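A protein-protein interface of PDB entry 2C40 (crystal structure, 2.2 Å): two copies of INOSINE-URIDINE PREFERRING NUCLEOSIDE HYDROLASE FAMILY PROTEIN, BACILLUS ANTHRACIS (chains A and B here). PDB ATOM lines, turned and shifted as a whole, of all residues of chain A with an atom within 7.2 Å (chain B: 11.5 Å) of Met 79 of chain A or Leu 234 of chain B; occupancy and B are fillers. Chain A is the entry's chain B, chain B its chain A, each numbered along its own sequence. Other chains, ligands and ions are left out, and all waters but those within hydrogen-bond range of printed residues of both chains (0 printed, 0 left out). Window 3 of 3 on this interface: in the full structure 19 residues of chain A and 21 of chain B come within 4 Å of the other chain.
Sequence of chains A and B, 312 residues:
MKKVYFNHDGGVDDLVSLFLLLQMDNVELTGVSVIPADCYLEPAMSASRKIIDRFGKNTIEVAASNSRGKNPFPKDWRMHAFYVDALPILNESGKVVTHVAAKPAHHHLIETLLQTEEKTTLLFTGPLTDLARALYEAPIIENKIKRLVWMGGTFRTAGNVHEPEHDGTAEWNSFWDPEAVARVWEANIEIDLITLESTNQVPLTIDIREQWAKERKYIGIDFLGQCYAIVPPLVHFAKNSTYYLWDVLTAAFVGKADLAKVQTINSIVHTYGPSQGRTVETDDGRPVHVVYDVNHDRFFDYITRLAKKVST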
ATOM      1  N   GLY A  10       2.639 -12.038 -26.083  1.00  0.00           N
ATOM      2  CA  GLY A  10       3.789 -12.854 -25.753  1.00  0.00           C
ATOM      3  C   GLY A  10       4.427 -12.770 -24.387  1.00  0.00           C
ATOM      4  O   GLY A  10       5.498 -13.374 -24.184  1.00  0.00           O
ATOM      5  N   ASP A  38       4.756  -6.570 -25.563  1.00  0.00           N
ATOM      6  CA  ASP A  38       5.407  -7.099 -24.378  1.00  0.00           C
ATOM      7  C   ASP A  38       6.201  -8.353 -24.702  1.00  0.00           C
ATOM      8  O   ASP A  38       6.351  -9.254 -23.861  1.00  0.00           O
ATOM      9  CB  ASP A  38       4.354  -7.426 -23.349  1.00  0.00           C
ATOM     10  CG  ASP A  38       4.901  -7.565 -21.970  1.00  0.00           C
ATOM     11  OD1 ASP A  38       4.111  -8.050 -21.140  1.00  0.00           O
ATOM     12  OD2 ASP A  38       6.064  -7.176 -21.733  1.00  0.00           O
ATOM     13  N   CYS A  39       6.773  -8.390 -25.894  1.00  0.00           N
ATOM     14  CA  CYS A  39       7.614  -9.504 -26.303  1.00  0.00           C
ATOM     15  C   CYS A  39       8.436  -9.112 -27.498  1.00  0.00           C
ATOM     16  O   CYS A  39       8.128  -8.132 -28.149  1.00  0.00           O
ATOM     17  CB  CYS A  39       6.773 -10.697 -26.655  1.00  0.00           C
ATOM     18  SG  CYS A  39       5.799 -10.539 -28.169  1.00  0.00           S
ATOM     19  N   TYR A  40       9.504  -9.872 -27.740  1.00  0.00           N
ATOM     20  CA  TYR A  40      10.122  -9.958 -29.032  1.00  0.00           C
ATOM     21  C   TYR A  40       9.345 -10.954 -29.853  1.00  0.00           C
ATOM     22  O   TYR A  40       8.911 -11.976 -29.321  1.00  0.00           O
ATOM     23  CB  TYR A  40      11.583 -10.367 -28.929  1.00  0.00           C
ATOM     24  CG  TYR A  40      12.442  -9.262 -28.366  1.00  0.00           C
ATOM     25  CD1 TYR A  40      12.491  -9.018 -26.984  1.00  0.00           C
ATOM     26  CD2 TYR A  40      13.126  -8.405 -29.207  1.00  0.00           C
ATOM     27  CE1 TYR A  40      13.275  -7.980 -26.440  1.00  0.00           C
ATOM     28  CE2 TYR A  40      13.899  -7.366 -28.699  1.00  0.00           C
ATOM     29  CZ  TYR A  40      13.978  -7.158 -27.293  1.00  0.00           C
ATOM     30  OH  TYR A  40      14.753  -6.118 -26.798  1.00  0.00           O
ATOM     31  N   PRO A  43      10.647 -15.257 -30.472  1.00  0.00           N
ATOM     32  CA  PRO A  43      10.371 -16.262 -29.415  1.00  0.00           C
ATOM     33  C   PRO A  43       8.875 -16.453 -29.109  1.00  0.00           C
ATOM     34  O   PRO A  43       8.430 -17.551 -28.846  1.00  0.00           O
ATOM     35  CB  PRO A  43      11.165 -15.723 -28.183  1.00  0.00           C
ATOM     36  CG  PRO A  43      11.226 -14.211 -28.441  1.00  0.00           C
ATOM     37  CD  PRO A  43      11.410 -14.109 -29.948  1.00  0.00           C
ATOM     38  N   PRO A  74       9.132  -1.942 -21.524  1.00  0.00           N
ATOM     39  CA  PRO A  74      10.497  -2.090 -21.007  1.00  0.00           C
ATOM     40  C   PRO A  74      11.163  -3.329 -21.575  1.00  0.00           C
ATOM     41  O   PRO A  74      10.497  -4.364 -21.714  1.00  0.00           O
ATOM     42  CB  PRO A  74      10.285  -2.239 -19.470  1.00  0.00           C
ATOM     43  CG  PRO A  74       8.999  -1.520 -19.227  1.00  0.00           C
ATOM     44  CD  PRO A  74       8.163  -1.893 -20.417  1.00  0.00           C
ATOM     45  N   LYS A  75      12.426  -3.218 -21.967  1.00  0.00           N
ATOM     46  CA  LYS A  75      13.117  -4.368 -22.590  1.00  0.00           C
ATOM     47  C   LYS A  75      13.095  -5.638 -21.692  1.00  0.00           C
ATOM     48  O   LYS A  75      12.903  -6.722 -22.219  1.00  0.00           O
ATOM     49  CB  LYS A  75      14.555  -4.011 -22.960  1.00  0.00           C
ATOM     50  CG  LYS A  75      15.364  -5.143 -23.605  1.00  0.00           C
ATOM     51  CD  LYS A  75      16.782  -4.710 -23.862  1.00  0.00           C
ATOM     52  CE  LYS A  75      17.584  -5.847 -24.429  1.00  0.00           C
ATOM     53  NZ  LYS A  75      18.847  -5.361 -24.954  1.00  0.00           N
ATOM     54  N   ASP A  76      13.240  -5.493 -20.363  1.00  0.00           N
ATOM     55  CA  ASP A  76      13.326  -6.632 -19.439  1.00  0.00           C
ATOM     56  C   ASP A  76      12.069  -7.513 -19.409  1.00  0.00           C
ATOM     57  O   ASP A  76      12.173  -8.741 -19.329  1.00  0.00           O
ATOM     58  CB  ASP A  76      13.650  -6.134 -17.998  1.00  0.00           C
ATOM     59  N   TRP A  77      10.894  -6.897 -19.479  1.00  0.00           N
ATOM     60  CA  TRP A  77       9.621  -7.630 -19.536  1.00  0.00           C
ATOM     61  C   TRP A  77       9.504  -8.390 -20.865  1.00  0.00           C
ATOM     62  O   TRP A  77       8.963  -9.507 -20.945  1.00  0.00           O
ATOM     63  CB  TRP A  77       8.420  -6.648 -19.411  1.00  0.00           C
ATOM     64  CG  TRP A  77       8.340  -5.782 -18.131  1.00  0.00           C
ATOM     65  CD1 TRP A  77       9.304  -5.652 -17.128  1.00  0.00           C
ATOM     66  CD2 TRP A  77       7.262  -4.892 -17.756  1.00  0.00           C
ATOM     67  NE1 TRP A  77       8.857  -4.771 -16.150  1.00  0.00           N
ATOM     68  CE2 TRP A  77       7.621  -4.284 -16.515  1.00  0.00           C
ATOM     69  CE3 TRP A  77       6.033  -4.566 -18.334  1.00  0.00           C
ATOM     70  CZ2 TRP A  77       6.789  -3.355 -15.858  1.00  0.00           C
ATOM     71  CZ3 TRP A  77       5.208  -3.630 -17.681  1.00  0.00           C
ATOM     72  CH2 TRP A  77       5.592  -3.047 -16.442  1.00  0.00           C
ATOM     73  N   ARG A  78      10.005  -7.754 -21.926  1.00  0.00           N
ATOM     74  CA  ARG A  78       9.949  -8.280 -23.283  1.00  0.00           C
ATOM     75  C   ARG A  78      10.715  -9.578 -23.534  1.00  0.00           C
ATOM     76  O   ARG A  78      10.367 -10.340 -24.428  1.00  0.00           O
ATOM     77  CB  ARG A  78      10.439  -7.194 -24.246  1.00  0.00           C
ATOM     78  CG  ARG A  78       9.528  -5.945 -24.277  1.00  0.00           C
ATOM     79  CD  ARG A  78       9.916  -5.080 -25.432  1.00  0.00           C
ATOM     80  NE  ARG A  78       9.635  -5.735 -26.715  1.00  0.00           N
ATOM     81  CZ  ARG A  78      10.278  -5.460 -27.843  1.00  0.00           C
ATOM     82  NH1 ARG A  78      11.236  -4.560 -27.853  1.00  0.00           N
ATOM     83  NH2 ARG A  78       9.990  -6.086 -28.962  1.00  0.00           N
ATOM     84  N   MET A  79      11.727  -9.834 -22.705  1.00  0.00           N
ATOM     85  CA  MET A  79      12.569 -11.056 -22.792  1.00  0.00           C
ATOM     86  C   MET A  79      11.892 -12.375 -22.451  1.00  0.00           C
ATOM     87  O   MET A  79      12.392 -13.419 -22.798  1.00  0.00           O
ATOM     88  CB  MET A  79      13.721 -10.921 -21.809  1.00  0.00           C
ATOM     89  CG  MET A  79      14.601  -9.737 -22.135  1.00  0.00           C
ATOM     90  SD  MET A  79      15.304  -9.855 -23.812  1.00  0.00           S
ATOM     91  CE  MET A  79      16.704 -10.907 -23.444  1.00  0.00           C
ATOM     92  N   HIS A  80      10.788 -12.319 -21.716  1.00  0.00           N
ATOM     93  CA  HIS A  80      10.205 -13.505 -21.062  1.00  0.00           C
ATOM     94  C   HIS A  80       9.864 -14.662 -22.027  1.00  0.00           C
ATOM     95  O   HIS A  80      10.066 -15.825 -21.708  1.00  0.00           O
ATOM     96  CB  HIS A  80       8.986 -13.069 -20.249  1.00  0.00           C
ATOM     97  CG  HIS A  80       9.353 -12.310 -18.998  1.00  0.00           C
ATOM     98  ND1 HIS A  80       8.424 -11.938 -18.058  1.00  0.00           N
ATOM     99  CD2 HIS A  80      10.565 -11.935 -18.500  1.00  0.00           C
ATOM    100  CE1 HIS A  80       9.032 -11.311 -17.064  1.00  0.00           C
ATOM    101  NE2 HIS A  80      10.329 -11.294 -17.310  1.00  0.00           N
ATOM    102  N   ALA A  81       9.440 -14.325 -23.232  1.00  0.00           N
ATOM    103  CA  ALA A  81       9.114 -15.350 -24.228  1.00  0.00           C
ATOM    104  C   ALA A  81      10.353 -16.164 -24.614  1.00  0.00           C
ATOM    105  O   ALA A  81      10.245 -17.362 -24.806  1.00  0.00           O
ATOM    106  CB  ALA A  81       8.398 -14.763 -25.434  1.00  0.00           C
ATOM    107  N   PHE A  82      11.544 -15.555 -24.660  1.00  0.00           N
ATOM    108  CA  PHE A  82      12.788 -16.324 -24.914  1.00  0.00           C
ATOM    109  C   PHE A  82      12.894 -17.519 -23.950  1.00  0.00           C
ATOM    110  O   PHE A  82      13.342 -18.626 -24.310  1.00  0.00           O
ATOM    111  CB  PHE A  82      14.026 -15.418 -24.781  1.00  0.00           C
ATOM    112  CG  PHE A  82      14.240 -14.510 -25.957  1.00  0.00           C
ATOM    113  CD1 PHE A  82      14.048 -13.147 -25.846  1.00  0.00           C
ATOM    114  CD2 PHE A  82      14.619 -15.033 -27.190  1.00  0.00           C
ATOM    115  CE1 PHE A  82      14.229 -12.316 -26.933  1.00  0.00           C
ATOM    116  CE2 PHE A  82      14.832 -14.194 -28.283  1.00  0.00           C
ATOM    117  CZ  PHE A  82      14.643 -12.840 -28.150  1.00  0.00           C
ATOM    118  N   TYR A  83      12.485 -17.289 -22.709  1.00  0.00           N
ATOM    119  CA  TYR A  83      12.576 -18.304 -21.669  1.00  0.00           C
ATOM    120  C   TYR A  83      11.518 -19.401 -21.883  1.00  0.00           C
ATOM    121  O   TYR A  83      11.823 -20.595 -21.856  1.00  0.00           O
ATOM    122  CB  TYR A  83      12.382 -17.618 -20.325  1.00  0.00           C
ATOM    123  CG  TYR A  83      13.239 -16.346 -20.135  1.00  0.00           C
ATOM    124  CD1 TYR A  83      12.806 -15.270 -19.318  1.00  0.00           C
ATOM    125  CD2 TYR A  83      14.496 -16.223 -20.756  1.00  0.00           C
ATOM    126  CE1 TYR A  83      13.616 -14.122 -19.115  1.00  0.00           C
ATOM    127  CE2 TYR A  83      15.286 -15.089 -20.588  1.00  0.00           C
ATOM    128  CZ  TYR A  83      14.841 -14.049 -19.781  1.00  0.00           C
ATOM    129  OH  TYR A  83      15.696 -12.963 -19.630  1.00  0.00           O
ATOM    130  N   VAL A  84      10.274 -18.976 -22.138  1.00  0.00           N
ATOM    131  CA  VAL A  84       9.190 -19.911 -22.348  1.00  0.00           C
ATOM    132  C   VAL A  84       9.499 -20.820 -23.574  1.00  0.00           C
ATOM    133  O   VAL A  84       9.398 -22.045 -23.484  1.00  0.00           O
ATOM    134  CB  VAL A  84       7.814 -19.217 -22.518  1.00  0.00           C
ATOM    135  CG1 VAL A  84       6.731 -20.260 -22.755  1.00  0.00           C
ATOM    136  CG2 VAL A  84       7.437 -18.359 -21.290  1.00  0.00           C
ATOM    137  N   ILE A 230       9.707 -17.827 -13.870  1.00  0.00           N
ATOM    138  CA  ILE A 230      10.279 -16.684 -14.599  1.00  0.00           C
ATOM    139  C   ILE A 230       9.862 -15.312 -14.000  1.00  0.00           C
ATOM    140  O   ILE A 230      10.547 -14.325 -14.136  1.00  0.00           O
ATOM    141  CB  ILE A 230       9.823 -16.807 -16.132  1.00  0.00           C
ATOM    142  CG1 ILE A 230       9.999 -18.298 -16.597  1.00  0.00           C
ATOM    143  CG2 ILE A 230      10.554 -15.849 -16.980  1.00  0.00           C
ATOM    144  CD1 ILE A 230      10.384 -18.699 -18.079  1.00  0.00           C
ATOM    145  N   ASP B  76      20.897  -7.855 -13.333  1.00  0.00           N
ATOM    146  CA  ASP B  76      20.017  -8.771 -14.118  1.00  0.00           C
ATOM    147  C   ASP B  76      20.573 -10.193 -14.155  1.00  0.00           C
ATOM    148  O   ASP B  76      19.815 -11.145 -14.142  1.00  0.00           O
ATOM    149  CB  ASP B  76      19.641  -8.214 -15.513  1.00  0.00           C
ATOM    150  N   TRP B  77      21.895 -10.334 -14.116  1.00  0.00           N
ATOM    151  CA  TRP B  77      22.536 -11.656 -13.971  1.00  0.00           C
ATOM    152  C   TRP B  77      22.239 -12.272 -12.597  1.00  0.00           C
ATOM    153  O   TRP B  77      21.939 -13.459 -12.453  1.00  0.00           O
ATOM    154  CB  TRP B  77      24.049 -11.491 -14.092  1.00  0.00           C
ATOM    155  CG  TRP B  77      24.535 -11.031 -15.428  1.00  0.00           C
ATOM    156  CD1 TRP B  77      23.782 -10.499 -16.468  1.00  0.00           C
ATOM    157  CD2 TRP B  77      25.905 -11.015 -15.870  1.00  0.00           C
ATOM    158  NE1 TRP B  77      24.620 -10.180 -17.516  1.00  0.00           N
ATOM    159  CE2 TRP B  77      25.918 -10.495 -17.177  1.00  0.00           C
ATOM    160  CE3 TRP B  77      27.116 -11.402 -15.282  1.00  0.00           C
ATOM    161  CZ2 TRP B  77      27.100 -10.340 -17.901  1.00  0.00           C
ATOM    162  CZ3 TRP B  77      28.284 -11.257 -16.002  1.00  0.00           C
ATOM    163  CH2 TRP B  77      28.273 -10.731 -17.294  1.00  0.00           C
ATOM    164  N   MET B  79      19.671 -12.134 -10.678  1.00  0.00           N
ATOM    165  CA  MET B  79      18.301 -12.584 -10.447  1.00  0.00           C
ATOM    166  C   MET B  79      18.085 -14.079 -10.701  1.00  0.00           C
ATOM    167  O   MET B  79      17.099 -14.643 -10.248  1.00  0.00           O
ATOM    168  CB  MET B  79      17.335 -11.806 -11.370  1.00  0.00           C
ATOM    169  CG  MET B  79      17.148 -10.330 -11.053  1.00  0.00           C
ATOM    170  SD  MET B  79      16.542  -9.943  -9.394  1.00  0.00           S
ATOM    171  CE  MET B  79      14.762 -10.161  -9.514  1.00  0.00           C
ATOM    172  N   HIS B  80      18.984 -14.713 -11.444  1.00  0.00           N
ATOM    173  CA  HIS B  80      18.735 -16.030 -12.046  1.00  0.00           C
ATOM    174  C   HIS B  80      18.393 -17.137 -11.042  1.00  0.00           C
ATOM    175  O   HIS B  80      17.562 -18.045 -11.349  1.00  0.00           O
ATOM    176  CB  HIS B  80      19.922 -16.433 -12.917  1.00  0.00           C
ATOM    177  CG  HIS B  80      20.018 -15.658 -14.192  1.00  0.00           C
ATOM    178  ND1 HIS B  80      21.069 -15.792 -15.068  1.00  0.00           N
ATOM    179  CD2 HIS B  80      19.210 -14.702 -14.716  1.00  0.00           C
ATOM    180  CE1 HIS B  80      20.880 -14.998 -16.109  1.00  0.00           C
ATOM    181  NE2 HIS B  80      19.754 -14.328 -15.923  1.00  0.00           N
ATOM    182  N   TYR B  83      14.739 -17.707 -10.150  1.00  0.00           N
ATOM    183  CA  TYR B  83      14.043 -18.524 -11.094  1.00  0.00           C
ATOM    184  C   TYR B  83      14.318 -19.966 -10.848  1.00  0.00           C
ATOM    185  O   TYR B  83      13.376 -20.743 -10.800  1.00  0.00           O
ATOM    186  CB  TYR B  83      14.359 -18.102 -12.541  1.00  0.00           C
ATOM    187  CG  TYR B  83      14.374 -16.582 -12.725  1.00  0.00           C
ATOM    188  CD1 TYR B  83      15.331 -15.960 -13.537  1.00  0.00           C
ATOM    189  CD2 TYR B  83      13.490 -15.763 -12.020  1.00  0.00           C
ATOM    190  CE1 TYR B  83      15.356 -14.570 -13.682  1.00  0.00           C
ATOM    191  CE2 TYR B  83      13.517 -14.364 -12.144  1.00  0.00           C
ATOM    192  CZ  TYR B  83      14.449 -13.786 -12.972  1.00  0.00           C
ATOM    193  OH  TYR B  83      14.460 -12.424 -13.116  1.00  0.00           O
ATOM    194  N   LEU B 204      27.776 -24.096 -25.375  1.00  0.00           N
ATOM    195  CA  LEU B 204      26.408 -24.620 -25.303  1.00  0.00           C
ATOM    196  C   LEU B 204      25.713 -24.079 -26.517  1.00  0.00           C
ATOM    197  O   LEU B 204      25.605 -22.856 -26.717  1.00  0.00           O
ATOM    198  CB  LEU B 204      25.628 -24.191 -24.087  1.00  0.00           C
ATOM    199  CG  LEU B 204      24.582 -25.156 -23.459  1.00  0.00           C
ATOM    200  CD1 LEU B 204      23.446 -24.338 -23.008  1.00  0.00           C
ATOM    201  CD2 LEU B 204      24.095 -26.287 -24.306  1.00  0.00           C
ATOM    202  N   THR B 205      25.178 -25.015 -27.273  1.00  0.00           N
ATOM    203  CA  THR B 205      24.677 -24.765 -28.578  1.00  0.00           C
ATOM    204  C   THR B 205      23.155 -25.095 -28.591  1.00  0.00           C
ATOM    205  O   THR B 205      22.661 -25.813 -27.723  1.00  0.00           O
ATOM    206  CB  THR B 205      25.599 -25.626 -29.471  1.00  0.00           C
ATOM    207  OG1 THR B 205      26.087 -24.862 -30.566  1.00  0.00           O
ATOM    208  CG2 THR B 205      24.977 -26.880 -29.893  1.00  0.00           C
ATOM    209  N   ILE B 206      22.416 -24.544 -29.544  1.00  0.00           N
ATOM    210  CA  ILE B 206      21.003 -24.891 -29.729  1.00  0.00           C
ATOM    211  C   ILE B 206      20.841 -26.413 -29.977  1.00  0.00           C
ATOM    212  O   ILE B 206      19.964 -27.046 -29.394  1.00  0.00           O
ATOM    213  CB  ILE B 206      20.343 -24.039 -30.911  1.00  0.00           C
ATOM    214  CG1 ILE B 206      20.189 -22.562 -30.531  1.00  0.00           C
ATOM    215  CG2 ILE B 206      18.993 -24.624 -31.365  1.00  0.00           C
ATOM    216  CD1 ILE B 206      20.126 -21.594 -31.816  1.00  0.00           C
ATOM    217  N   ARG B 209      21.002 -28.056 -26.608  1.00  0.00           N
ATOM    218  CA  ARG B 209      19.756 -27.764 -25.887  1.00  0.00           C
ATOM    219  C   ARG B 209      18.627 -28.617 -26.434  1.00  0.00           C
ATOM    220  O   ARG B 209      17.892 -29.197 -25.667  1.00  0.00           O
ATOM    221  CB  ARG B 209      19.413 -26.284 -25.988  1.00  0.00           C
ATOM    222  CG  ARG B 209      20.388 -25.312 -25.260  1.00  0.00           C
ATOM    223  CD  ARG B 209      20.200 -23.860 -25.796  1.00  0.00           C
ATOM    224  NE  ARG B 209      21.179 -22.930 -25.248  1.00  0.00           N
ATOM    225  CZ  ARG B 209      21.011 -22.178 -24.151  1.00  0.00           C
ATOM    226  NH1 ARG B 209      19.848 -22.186 -23.460  1.00  0.00           N
ATOM    227  NH2 ARG B 209      22.027 -21.395 -23.733  1.00  0.00           N
ATOM    228  N   TYR B 228      18.721 -24.063 -18.180  1.00  0.00           N
ATOM    229  CA  TYR B 228      19.286 -23.318 -19.313  1.00  0.00           C
ATOM    230  C   TYR B 228      18.299 -22.494 -20.153  1.00  0.00           C
ATOM    231  O   TYR B 228      18.717 -21.661 -20.935  1.00  0.00           O
ATOM    232  CB  TYR B 228      20.148 -24.259 -20.156  1.00  0.00           C
ATOM    233  CG  TYR B 228      21.464 -24.521 -19.440  1.00  0.00           C
ATOM    234  CD1 TYR B 228      21.814 -25.795 -18.994  1.00  0.00           C
ATOM    235  CD2 TYR B 228      22.320 -23.448 -19.136  1.00  0.00           C
ATOM    236  CE1 TYR B 228      22.993 -26.001 -18.333  1.00  0.00           C
ATOM    237  CE2 TYR B 228      23.452 -23.626 -18.460  1.00  0.00           C
ATOM    238  CZ  TYR B 228      23.809 -24.911 -18.035  1.00  0.00           C
ATOM    239  OH  TYR B 228      24.999 -25.077 -17.364  1.00  0.00           O
ATOM    240  N   ALA B 229      17.002 -22.697 -19.944  1.00  0.00           N
ATOM    241  CA  ALA B 229      15.943 -21.907 -20.544  1.00  0.00           C
ATOM    242  C   ALA B 229      15.996 -20.457 -20.071  1.00  0.00           C
ATOM    243  O   ALA B 229      15.593 -19.523 -20.755  1.00  0.00           O
ATOM    244  CB  ALA B 229      14.612 -22.512 -20.140  1.00  0.00           C
ATOM    245  N   ILE B 230      16.428 -20.318 -18.836  1.00  0.00           N
ATOM    246  CA  ILE B 230      16.668 -19.040 -18.125  1.00  0.00           C
ATOM    247  C   ILE B 230      17.780 -18.180 -18.774  1.00  0.00           C
ATOM    248  O   ILE B 230      17.888 -16.992 -18.574  1.00  0.00           O
ATOM    249  CB  ILE B 230      17.026 -19.426 -16.638  1.00  0.00           C
ATOM    250  CG1 ILE B 230      15.725 -19.895 -15.920  1.00  0.00           C
ATOM    251  CG2 ILE B 230      17.755 -18.340 -15.940  1.00  0.00           C
ATOM    252  CD1 ILE B 230      15.850 -20.502 -14.441  1.00  0.00           C
ATOM    253  N   VAL B 231      18.610 -18.810 -19.567  1.00  0.00           N
ATOM    254  CA  VAL B 231      19.701 -18.155 -20.214  1.00  0.00           C
ATOM    255  C   VAL B 231      19.707 -18.650 -21.697  1.00  0.00           C
ATOM    256  O   VAL B 231      20.672 -19.239 -22.174  1.00  0.00           O
ATOM    257  CB  VAL B 231      20.943 -18.471 -19.337  1.00  0.00           C
ATOM    258  CG1 VAL B 231      21.669 -19.734 -19.740  1.00  0.00           C
ATOM    259  CG2 VAL B 231      21.848 -17.270 -19.209  1.00  0.00           C
ATOM    260  N   PRO B 232      18.595 -18.419 -22.414  1.00  0.00           N
ATOM    261  CA  PRO B 232      18.330 -19.047 -23.687  1.00  0.00           C
ATOM    262  C   PRO B 232      19.023 -18.350 -24.887  1.00  0.00           C
ATOM    263  O   PRO B 232      19.585 -17.252 -24.741  1.00  0.00           O
ATOM    264  CB  PRO B 232      16.819 -18.880 -23.811  1.00  0.00           C
ATOM    265  CG  PRO B 232      16.613 -17.561 -23.285  1.00  0.00           C
ATOM    266  CD  PRO B 232      17.527 -17.470 -22.091  1.00  0.00           C
ATOM    267  N   PRO B 233      18.959 -18.982 -26.071  1.00  0.00           N
ATOM    268  CA  PRO B 233      19.511 -18.330 -27.256  1.00  0.00           C
ATOM    269  C   PRO B 233      18.597 -17.134 -27.654  1.00  0.00           C
ATOM    270  O   PRO B 233      17.381 -17.244 -27.570  1.00  0.00           O
ATOM    271  CB  PRO B 233      19.536 -19.456 -28.307  1.00  0.00           C
ATOM    272  CG  PRO B 233      19.211 -20.757 -27.545  1.00  0.00           C
ATOM    273  CD  PRO B 233      18.360 -20.299 -26.384  1.00  0.00           C
ATOM    274  N   LEU B 234      19.178 -16.013 -28.059  1.00  0.00           N
ATOM    275  CA  LEU B 234      18.427 -14.783 -28.327  1.00  0.00           C
ATOM    276  C   LEU B 234      18.259 -14.420 -29.822  1.00  0.00           C
ATOM    277  O   LEU B 234      18.588 -15.234 -30.695  1.00  0.00           O
ATOM    278  CB  LEU B 234      19.061 -13.626 -27.543  1.00  0.00           C
ATOM    279  CG  LEU B 234      19.139 -13.835 -26.022  1.00  0.00           C
ATOM    280  CD1 LEU B 234      19.788 -12.641 -25.360  1.00  0.00           C
ATOM    281  CD2 LEU B 234      17.765 -14.100 -25.421  1.00  0.00           C
ATOM    282  N   TYR B 243      26.815 -19.691 -25.840  1.00  0.00           N
ATOM    283  CA  TYR B 243      27.011 -19.582 -24.386  1.00  0.00           C
ATOM    284  C   TYR B 243      27.958 -20.687 -23.892  1.00  0.00           C
ATOM    285  O   TYR B 243      27.906 -21.813 -24.323  1.00  0.00           O
ATOM    286  CB  TYR B 243      25.618 -19.668 -23.736  1.00  0.00           C
ATOM    287  CG  TYR B 243      25.514 -19.780 -22.248  1.00  0.00           C
ATOM    288  CD1 TYR B 243      25.863 -20.969 -21.576  1.00  0.00           C
ATOM    289  CD2 TYR B 243      24.963 -18.740 -21.506  1.00  0.00           C
ATOM    290  CE1 TYR B 243      25.730 -21.086 -20.199  1.00  0.00           C
ATOM    291  CE2 TYR B 243      24.837 -18.833 -20.109  1.00  0.00           C
ATOM    292  CZ  TYR B 243      25.199 -20.000 -19.467  1.00  0.00           C
ATOM    293  OH  TYR B 243      25.015 -20.077 -18.102  1.00  0.00           O
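Of the 17 printed residues of chain B, 6 touch a printed residue of chain A. Printed residues of chain B that touch a printed residue of chain A: Tyr 83, Ala 229, Ile 230, Pro 232, Pro 233 and Leu 234. Hydrophobic or aromatic side chains of chain B within 4 Å of the printed part of chain A: Tyr 83, Ala 229, Pro 232 and Leu 234.
Tyr 83 of chain A touches Ile 230 of chain B, and with the chains exchanged Ile 230 of chain A touches Tyr 83 of chain B. 6 positions are printed for both chains.
Met 79 of chain A touches Leu 234 of chain B (CE to CD2, 3.9 Å). Phe 82 of chain A touches Pro 232 of chain B. CD2 of Phe 82 of chain A touches O of Pro 233 of chain B (3.6 Å). CG of Phe 82 of chain A touches CD2 of Leu 234 of chain B (3.6 Å). Ala 229 of chain B touches Tyr 83 of chain A. Ile 230 of chain B touches Tyr 83 of chain A (O to CE2, 3.8 Å). CD2 of Tyr 83 of chain A touches CD of Pro 232 of chain B, at 3.5 Å. Ile 230 of chain A touches Tyr 83 of chain B (O to CE2, 3.6 Å).
Leu 234 of chain B touches two residues of chain A. No residue of chain B comes within 4 Å of Lys 75 of chain A. No residue of chain B comes within 4 Å of His 80 of chain A. No residue of chain B comes within 4 Å of Ala 81 of chain A. Phe 82 of chain A touches three residues of chain B. Tyr 83 of chain A touches just these residues of chain B: Ala 229, Ile 230 and Pro 232. Printed residues of chain A within 4 Å of Ala 229 of chain B: Tyr 83 (3.4 Å). Of the printed residues of chain A, Ile 230 of chain B touches Tyr 83. Of the printed residues of chain A, Pro 232 of chain B touches Phe 82 (3.5 Å) and Tyr 83 (3.5 Å). Of the printed residues of chain A, Tyr 83 of chain B touches Ile 230 (3.6 Å). Of the printed residues of chain A, Pro 233 of chain B touches Phe 82 (3.6 Å). The nearest residue of chain B that does not touch Met 79 of chain A is Pro 232 of chain B (5.9 Å). The nearest residue of chain A that does not touch Leu 234 of chain B is Tyr 83 of chain A (5.5 Å). The nearest printed residue of chain A that does not touch Tyr 83 of chain B is Tyr 83 of chain A (5.7 Å).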
